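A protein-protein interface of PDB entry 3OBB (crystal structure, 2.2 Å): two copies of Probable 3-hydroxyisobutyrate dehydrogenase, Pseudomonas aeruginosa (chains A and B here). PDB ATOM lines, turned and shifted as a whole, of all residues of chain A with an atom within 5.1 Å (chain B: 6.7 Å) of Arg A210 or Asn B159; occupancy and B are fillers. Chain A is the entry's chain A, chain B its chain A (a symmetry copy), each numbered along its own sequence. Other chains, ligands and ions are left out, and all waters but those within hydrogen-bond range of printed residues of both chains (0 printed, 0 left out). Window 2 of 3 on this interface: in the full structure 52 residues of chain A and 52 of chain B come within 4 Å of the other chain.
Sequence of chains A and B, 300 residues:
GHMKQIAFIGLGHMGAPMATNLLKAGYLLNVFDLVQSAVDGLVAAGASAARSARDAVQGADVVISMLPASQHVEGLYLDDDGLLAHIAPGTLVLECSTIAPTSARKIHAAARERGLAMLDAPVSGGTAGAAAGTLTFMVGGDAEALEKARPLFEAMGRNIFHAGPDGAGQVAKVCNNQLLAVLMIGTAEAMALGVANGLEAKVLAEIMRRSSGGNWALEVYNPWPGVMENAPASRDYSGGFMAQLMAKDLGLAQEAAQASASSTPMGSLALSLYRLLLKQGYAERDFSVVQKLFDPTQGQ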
ATOM      1  N   ALA A 205      -3.650  11.736  10.717  1.00  0.00           N
ATOM      2  CA  ALA A 205      -2.686  10.644  10.590  1.00  0.00           C
ATOM      3  C   ALA A 205      -1.247  11.150  10.673  1.00  0.00           C
ATOM      4  O   ALA A 205      -0.425  10.579  11.392  1.00  0.00           O
ATOM      5  CB  ALA A 205      -2.899   9.846   9.261  1.00  0.00           C
ATOM      6  N   GLU A 206      -0.939  12.228   9.943  1.00  0.00           N
ATOM      7  CA  GLU A 206       0.437  12.735   9.920  1.00  0.00           C
ATOM      8  C   GLU A 206       0.825  13.258  11.316  1.00  0.00           C
ATOM      9  O   GLU A 206       1.936  12.998  11.805  1.00  0.00           O
ATOM     10  CB  GLU A 206       0.658  13.801   8.818  1.00  0.00           C
ATOM     11  CG  GLU A 206       2.107  14.365   8.834  1.00  0.00           C
ATOM     12  CD  GLU A 206       2.347  15.707   8.093  1.00  0.00           C
ATOM     13  OE1 GLU A 206       1.369  16.319   7.575  1.00  0.00           O
ATOM     14  OE2 GLU A 206       3.536  16.151   8.062  1.00  0.00           O
ATOM     15  N   ILE A 207      -0.091  13.990  11.958  1.00  0.00           N
ATOM     16  CA  ILE A 207       0.190  14.587  13.278  1.00  0.00           C
ATOM     17  C   ILE A 207       0.527  13.507  14.303  1.00  0.00           C
ATOM     18  O   ILE A 207       1.552  13.576  14.983  1.00  0.00           O
ATOM     19  CB  ILE A 207      -0.989  15.482  13.753  1.00  0.00           C
ATOM     20  CG1 ILE A 207      -0.996  16.802  12.985  1.00  0.00           C
ATOM     21  CG2 ILE A 207      -0.912  15.796  15.227  1.00  0.00           C
ATOM     22  CD1 ILE A 207      -2.347  17.506  12.975  1.00  0.00           C
ATOM     23  N   MET A 208      -0.310  12.474  14.362  1.00  0.00           N
ATOM     24  CA  MET A 208      -0.143  11.418  15.360  1.00  0.00           C
ATOM     25  C   MET A 208       1.069  10.579  15.054  1.00  0.00           C
ATOM     26  O   MET A 208       1.805  10.214  15.984  1.00  0.00           O
ATOM     27  CB  MET A 208      -1.395  10.553  15.496  1.00  0.00           C
ATOM     28  CG  MET A 208      -2.590  11.317  16.011  1.00  0.00           C
ATOM     29  SD  MET A 208      -4.031  10.179  16.591  1.00  0.00           S
ATOM     30  CE  MET A 208      -4.327   9.201  14.900  1.00  0.00           C
ATOM     31  N   ARG A 209       1.302  10.296  13.764  1.00  0.00           N
ATOM     32  CA  ARG A 209       2.444   9.468  13.339  1.00  0.00           C
ATOM     33  C   ARG A 209       3.742  10.105  13.788  1.00  0.00           C
ATOM     34  O   ARG A 209       4.706   9.414  14.181  1.00  0.00           O
ATOM     35  CB  ARG A 209       2.476   9.246  11.805  1.00  0.00           C
ATOM     36  CG  ARG A 209       3.818   8.655  11.322  1.00  0.00           C
ATOM     37  CD  ARG A 209       3.908   8.408   9.801  1.00  0.00           C
ATOM     38  NE  ARG A 209       3.688   9.645   9.059  1.00  0.00           N
ATOM     39  CZ  ARG A 209       4.635  10.529   8.770  1.00  0.00           C
ATOM     40  NH1 ARG A 209       5.899  10.267   9.126  1.00  0.00           N
ATOM     41  NH2 ARG A 209       4.308  11.668   8.097  1.00  0.00           N
ATOM     42  N   ARG A 210       3.766  11.434  13.739  1.00  0.00           N
ATOM     43  CA  ARG A 210       4.982  12.191  14.023  1.00  0.00           C
ATOM     44  C   ARG A 210       5.078  12.641  15.496  1.00  0.00           C
ATOM     45  O   ARG A 210       6.033  13.326  15.877  1.00  0.00           O
ATOM     46  CB  ARG A 210       5.041  13.423  13.128  1.00  0.00           C
ATOM     47  CG  ARG A 210       5.312  13.170  11.658  1.00  0.00           C
ATOM     48  CD  ARG A 210       6.412  14.173  11.288  1.00  0.00           C
ATOM     49  NE  ARG A 210       5.931  15.116  10.326  1.00  0.00           N
ATOM     50  CZ  ARG A 210       6.601  16.176   9.882  1.00  0.00           C
ATOM     51  NH1 ARG A 210       7.814  16.488  10.346  1.00  0.00           N
ATOM     52  NH2 ARG A 210       6.026  16.937   8.958  1.00  0.00           N
ATOM     53  N   SER A 211       4.103  12.239  16.305  1.00  0.00           N
ATOM     54  CA  SER A 211       4.032  12.651  17.695  1.00  0.00           C
ATOM     55  C   SER A 211       3.993  11.456  18.659  1.00  0.00           C
ATOM     56  O   SER A 211       4.313  10.320  18.270  1.00  0.00           O
ATOM     57  CB  SER A 211       2.857  13.614  17.911  1.00  0.00           C
ATOM     58  OG  SER A 211       2.930  14.665  16.962  1.00  0.00           O
ATOM     59  N   SER A 212       3.628  11.717  19.915  1.00  0.00           N
ATOM     60  CA  SER A 212       3.664  10.664  20.957  1.00  0.00           C
ATOM     61  C   SER A 212       2.616   9.549  20.732  1.00  0.00           C
ATOM     62  O   SER A 212       2.724   8.491  21.313  1.00  0.00           O
ATOM     63  CB  SER A 212       3.550  11.283  22.350  1.00  0.00           C
ATOM     64  OG  SER A 212       2.348  12.023  22.438  1.00  0.00           O
ATOM     65  N   THR B 134      11.294  22.764  21.582  1.00  0.00           N
ATOM     66  CA  THR B 134      11.110  21.715  20.535  1.00  0.00           C
ATOM     67  C   THR B 134       9.692  21.115  20.533  1.00  0.00           C
ATOM     68  O   THR B 134       9.440  20.044  19.944  1.00  0.00           O
ATOM     69  CB  THR B 134      12.092  20.552  20.735  1.00  0.00           C
ATOM     70  OG1 THR B 134      11.869  19.977  22.037  1.00  0.00           O
ATOM     71  CG2 THR B 134      13.553  21.021  20.620  1.00  0.00           C
ATOM     72  N   LEU B 135       8.786  21.812  21.208  1.00  0.00           N
ATOM     73  CA  LEU B 135       7.394  21.407  21.340  1.00  0.00           C
ATOM     74  C   LEU B 135       6.713  21.221  19.992  1.00  0.00           C
ATOM     75  O   LEU B 135       7.039  21.884  19.022  1.00  0.00           O
ATOM     76  CB  LEU B 135       6.624  22.484  22.120  1.00  0.00           C
ATOM     77  CG  LEU B 135       6.921  22.645  23.597  1.00  0.00           C
ATOM     78  CD1 LEU B 135       6.111  23.838  24.139  1.00  0.00           C
ATOM     79  CD2 LEU B 135       6.610  21.344  24.344  1.00  0.00           C
ATOM     80  N   THR B 136       5.747  20.334  19.918  1.00  0.00           N
ATOM     81  CA  THR B 136       4.884  20.389  18.732  1.00  0.00           C
ATOM     82  C   THR B 136       3.602  21.140  19.050  1.00  0.00           C
ATOM     83  O   THR B 136       3.050  21.020  20.130  1.00  0.00           O
ATOM     84  CB  THR B 136       4.727  19.037  17.935  1.00  0.00           C
ATOM     85  OG1 THR B 136       3.336  18.761  17.597  1.00  0.00           O
ATOM     86  CG2 THR B 136       5.356  17.917  18.646  1.00  0.00           C
ATOM     87  N   PHE B 137       3.196  21.983  18.122  1.00  0.00           N
ATOM     88  CA  PHE B 137       1.951  22.666  18.276  1.00  0.00           C
ATOM     89  C   PHE B 137       0.966  22.038  17.351  1.00  0.00           C
ATOM     90  O   PHE B 137       1.305  21.708  16.214  1.00  0.00           O
ATOM     91  CB  PHE B 137       2.113  24.150  17.952  1.00  0.00           C
ATOM     92  CG  PHE B 137       2.894  24.906  18.982  1.00  0.00           C
ATOM     93  CD1 PHE B 137       4.287  24.989  18.897  1.00  0.00           C
ATOM     94  CD2 PHE B 137       2.242  25.538  20.045  1.00  0.00           C
ATOM     95  CE1 PHE B 137       5.020  25.707  19.824  1.00  0.00           C
ATOM     96  CE2 PHE B 137       2.957  26.257  20.993  1.00  0.00           C
ATOM     97  CZ  PHE B 137       4.360  26.358  20.884  1.00  0.00           C
ATOM     98  N   MET B 138      -0.260  21.901  17.834  1.00  0.00           N
ATOM     99  CA  MET B 138      -1.370  21.400  17.020  1.00  0.00           C
ATOM    100  C   MET B 138      -2.439  22.479  16.981  1.00  0.00           C
ATOM    101  O   MET B 138      -3.057  22.814  17.988  1.00  0.00           O
ATOM    102  CB  MET B 138      -1.913  20.102  17.595  1.00  0.00           C
ATOM    103  CG  MET B 138      -0.857  19.027  17.677  1.00  0.00           C
ATOM    104  SD  MET B 138      -1.506  17.460  18.617  1.00  0.00           S
ATOM    105  CE  MET B 138       0.102  16.367  18.593  1.00  0.00           C
ATOM    106  N   PHE B 153       5.488  30.474  17.424  1.00  0.00           N
ATOM    107  CA  PHE B 153       5.494  29.011  17.506  1.00  0.00           C
ATOM    108  C   PHE B 153       6.883  28.475  17.238  1.00  0.00           C
ATOM    109  O   PHE B 153       7.326  27.545  17.900  1.00  0.00           O
ATOM    110  CB  PHE B 153       4.555  28.423  16.463  1.00  0.00           C
ATOM    111  CG  PHE B 153       3.103  28.617  16.764  1.00  0.00           C
ATOM    112  CD1 PHE B 153       2.204  28.881  15.739  1.00  0.00           C
ATOM    113  CD2 PHE B 153       2.629  28.543  18.060  1.00  0.00           C
ATOM    114  CE1 PHE B 153       0.842  29.038  15.995  1.00  0.00           C
ATOM    115  CE2 PHE B 153       1.274  28.721  18.333  1.00  0.00           C
ATOM    116  CZ  PHE B 153       0.376  28.964  17.286  1.00  0.00           C
ATOM    117  N   GLY B 157       8.797  26.137  19.793  1.00  0.00           N
ATOM    118  CA  GLY B 157       8.540  24.782  19.319  1.00  0.00           C
ATOM    119  C   GLY B 157       9.216  24.421  18.018  1.00  0.00           C
ATOM    120  O   GLY B 157      10.013  25.200  17.492  1.00  0.00           O
ATOM    121  N   ARG B 158       8.934  23.213  17.524  1.00  0.00           N
ATOM    122  CA  ARG B 158       9.586  22.719  16.327  1.00  0.00           C
ATOM    123  C   ARG B 158       8.578  22.276  15.278  1.00  0.00           C
ATOM    124  O   ARG B 158       8.476  22.925  14.245  1.00  0.00           O
ATOM    125  CB  ARG B 158      10.639  21.659  16.645  1.00  0.00           C
ATOM    126  CG  ARG B 158      11.193  20.926  15.403  1.00  0.00           C
ATOM    127  CD  ARG B 158      12.652  20.486  15.600  1.00  0.00           C
ATOM    128  NE  ARG B 158      12.792  19.372  16.539  1.00  0.00           N
ATOM    129  CZ  ARG B 158      13.895  19.116  17.241  1.00  0.00           C
ATOM    130  NH1 ARG B 158      13.917  18.086  18.082  1.00  0.00           N
ATOM    131  NH2 ARG B 158      14.975  19.885  17.107  1.00  0.00           N
ATOM    132  N   ASN B 159       7.840  21.194  15.503  1.00  0.00           N
ATOM    133  CA  ASN B 159       6.812  20.830  14.529  1.00  0.00           C
ATOM    134  C   ASN B 159       5.564  21.662  14.728  1.00  0.00           C
ATOM    135  O   ASN B 159       5.033  21.733  15.833  1.00  0.00           O
ATOM    136  CB  ASN B 159       6.440  19.354  14.609  1.00  0.00           C
ATOM    137  CG  ASN B 159       7.517  18.463  14.061  1.00  0.00           C
ATOM    138  OD1 ASN B 159       8.401  18.921  13.328  1.00  0.00           O
ATOM    139  ND2 ASN B 159       7.461  17.174  14.418  1.00  0.00           N
ATOM    140  N   ILE B 160       5.084  22.266  13.651  1.00  0.00           N
ATOM    141  CA  ILE B 160       3.879  23.072  13.742  1.00  0.00           C
ATOM    142  C   ILE B 160       2.871  22.552  12.744  1.00  0.00           C
ATOM    143  O   ILE B 160       3.040  22.684  11.530  1.00  0.00           O
ATOM    144  CB  ILE B 160       4.161  24.616  13.600  1.00  0.00           C
ATOM    145  CG1 ILE B 160       5.229  25.055  14.610  1.00  0.00           C
ATOM    146  CG2 ILE B 160       2.899  25.417  13.839  1.00  0.00           C
ATOM    147  CD1 ILE B 160       6.140  26.081  14.099  1.00  0.00           C
ATOM    148  N   PHE B 161       1.818  21.941  13.270  1.00  0.00           N
ATOM    149  CA  PHE B 161       0.795  21.390  12.423  1.00  0.00           C
ATOM    150  C   PHE B 161      -0.457  22.232  12.451  1.00  0.00           C
ATOM    151  O   PHE B 161      -0.909  22.620  13.532  1.00  0.00           O
ATOM    152  CB  PHE B 161       0.456  19.962  12.865  1.00  0.00           C
ATOM    153  CG  PHE B 161       1.606  19.017  12.764  1.00  0.00           C
ATOM    154  CD1 PHE B 161       2.328  18.654  13.902  1.00  0.00           C
ATOM    155  CD2 PHE B 161       1.973  18.470  11.539  1.00  0.00           C
ATOM    156  CE1 PHE B 161       3.374  17.753  13.827  1.00  0.00           C
ATOM    157  CE2 PHE B 161       3.052  17.585  11.450  1.00  0.00           C
ATOM    158  CZ  PHE B 161       3.757  17.232  12.604  1.00  0.00           C
ATOM    159  N   ASN B 176      -4.448  12.193  19.882  1.00  0.00           N
ATOM    160  CA  ASN B 176      -3.054  11.805  19.980  1.00  0.00           C
ATOM    161  C   ASN B 176      -2.755  11.288  21.368  1.00  0.00           C
ATOM    162  O   ASN B 176      -2.163  10.247  21.488  1.00  0.00           O
ATOM    163  CB  ASN B 176      -2.109  12.970  19.677  1.00  0.00           C
ATOM    164  CG  ASN B 176      -0.665  12.589  19.883  1.00  0.00           C
ATOM    165  OD1 ASN B 176      -0.027  12.074  18.971  1.00  0.00           O
ATOM    166  ND2 ASN B 176      -0.148  12.780  21.124  1.00  0.00           N
ATOM    167  N   TRP B 216       5.871   4.667  19.799  1.00  0.00           N
ATOM    168  CA  TRP B 216       6.567   5.747  20.460  1.00  0.00           C
ATOM    169  C   TRP B 216       7.096   5.369  21.862  1.00  0.00           C
ATOM    170  O   TRP B 216       8.235   5.696  22.197  1.00  0.00           O
ATOM    171  CB  TRP B 216       5.635   6.930  20.566  1.00  0.00           C
ATOM    172  CG  TRP B 216       6.295   8.198  21.060  1.00  0.00           C
ATOM    173  CD1 TRP B 216       6.960   9.119  20.299  1.00  0.00           C
ATOM    174  CD2 TRP B 216       6.308   8.708  22.436  1.00  0.00           C
ATOM    175  NE1 TRP B 216       7.354  10.180  21.107  1.00  0.00           N
ATOM    176  CE2 TRP B 216       6.971   9.950  22.408  1.00  0.00           C
ATOM    177  CE3 TRP B 216       5.805   8.228  23.664  1.00  0.00           C
ATOM    178  CZ2 TRP B 216       7.162  10.733  23.574  1.00  0.00           C
ATOM    179  CZ3 TRP B 216       5.985   8.990  24.817  1.00  0.00           C
ATOM    180  CH2 TRP B 216       6.647  10.236  24.763  1.00  0.00           C
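ND2 of Asn B176 lies within hydrogen-bond range of OG of Ser A212, at 2.9 Å.
The side-chain carboxylate of Glu A206 is in salt-bridge range of the guanidinium group of Arg A210 (2.8 Å). O of Ile A207 sits at hydrogen-bond distance from OG of Ser A211, at 2.6 Å. N of Phe B137 lies within hydrogen-bond range of O of Asn B159 (2.9 Å). The backbone carbonyl oxygen (O) of Phe B137 is in hydrogen-bond range of the backbone NH (N) of Phe B161 (3.0 Å).
Glu A206 touches Phe B161 (OE2 to CE2, 3.7 Å). Met B138 touches Ile A207 (CE to CG2, 3.6 Å). CG of Phe B161 touches CG1 of Ile A207, at 3.4 Å. Met A208 touches Asn B176. Arg A210 touches Asn B159 (NH1 to OD1, 3.9 Å). NE of Arg A210 touches CZ of Phe B161 (3.8 Å). Ser A211 touches Met B138 (OG to CE, 3.7 Å). Asn B176 touches Ser A211 (OD1 to CB, 3.4 Å). O of Ser A211 touches CD1 of Trp B216, 3.5 Å away. Trp B216 touches Ser A212.
Ala A205 touches none of the printed residues of chain B. Printed residues of chain B within 4 Å of Ile A207: Met B138 and Phe B161. Of the printed residues of chain B, Met A208 touches Asn B176. Arg A210 touches just these residues of chain B: Asn B159 and Phe B161. Phe B137 touches none of the printed residues of chain A. Of the printed residues of chain A, Met B138 touches Ile A207 (3.6 Å) and Ser A211 (3.7 Å). Asn B159 touches just one residue of chain A: Arg A210 (3.9 Å). Of the printed residues of chain A, Asn B176 touches Met A208, Ser A211 and Ser A212. Of the printed residues of chain A, Trp B216 touches Ser A211 (3.5 Å) and Ser A212 (3.4 Å). The nearest printed residue of chain A that does not touch Asn B159 is Ser A211 (5.8 Å). The nearest printed residue of chain A that does not touch Phe B161 is Ser A211 (4.4 Å).
Hydrophobic or aromatic side chains of chain A within 4 Å of the printed part of chain B: Ile A207 and Met A208. Along chain A the printed residues that touch a printed residue of chain B span positions 206 to 212. Of the 13 printed residues of chain B, 5 touch a printed residue of chain A. Printed residues of chain B that touch a printed residue of chain A: Met B138, Asn B159, Phe B161, Asn B176 and Trp B216.
No position is printed for both chains. Of the 11 pairs that touch across the chains among the printed residues, none has its exchanged pair printed and touching as well.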
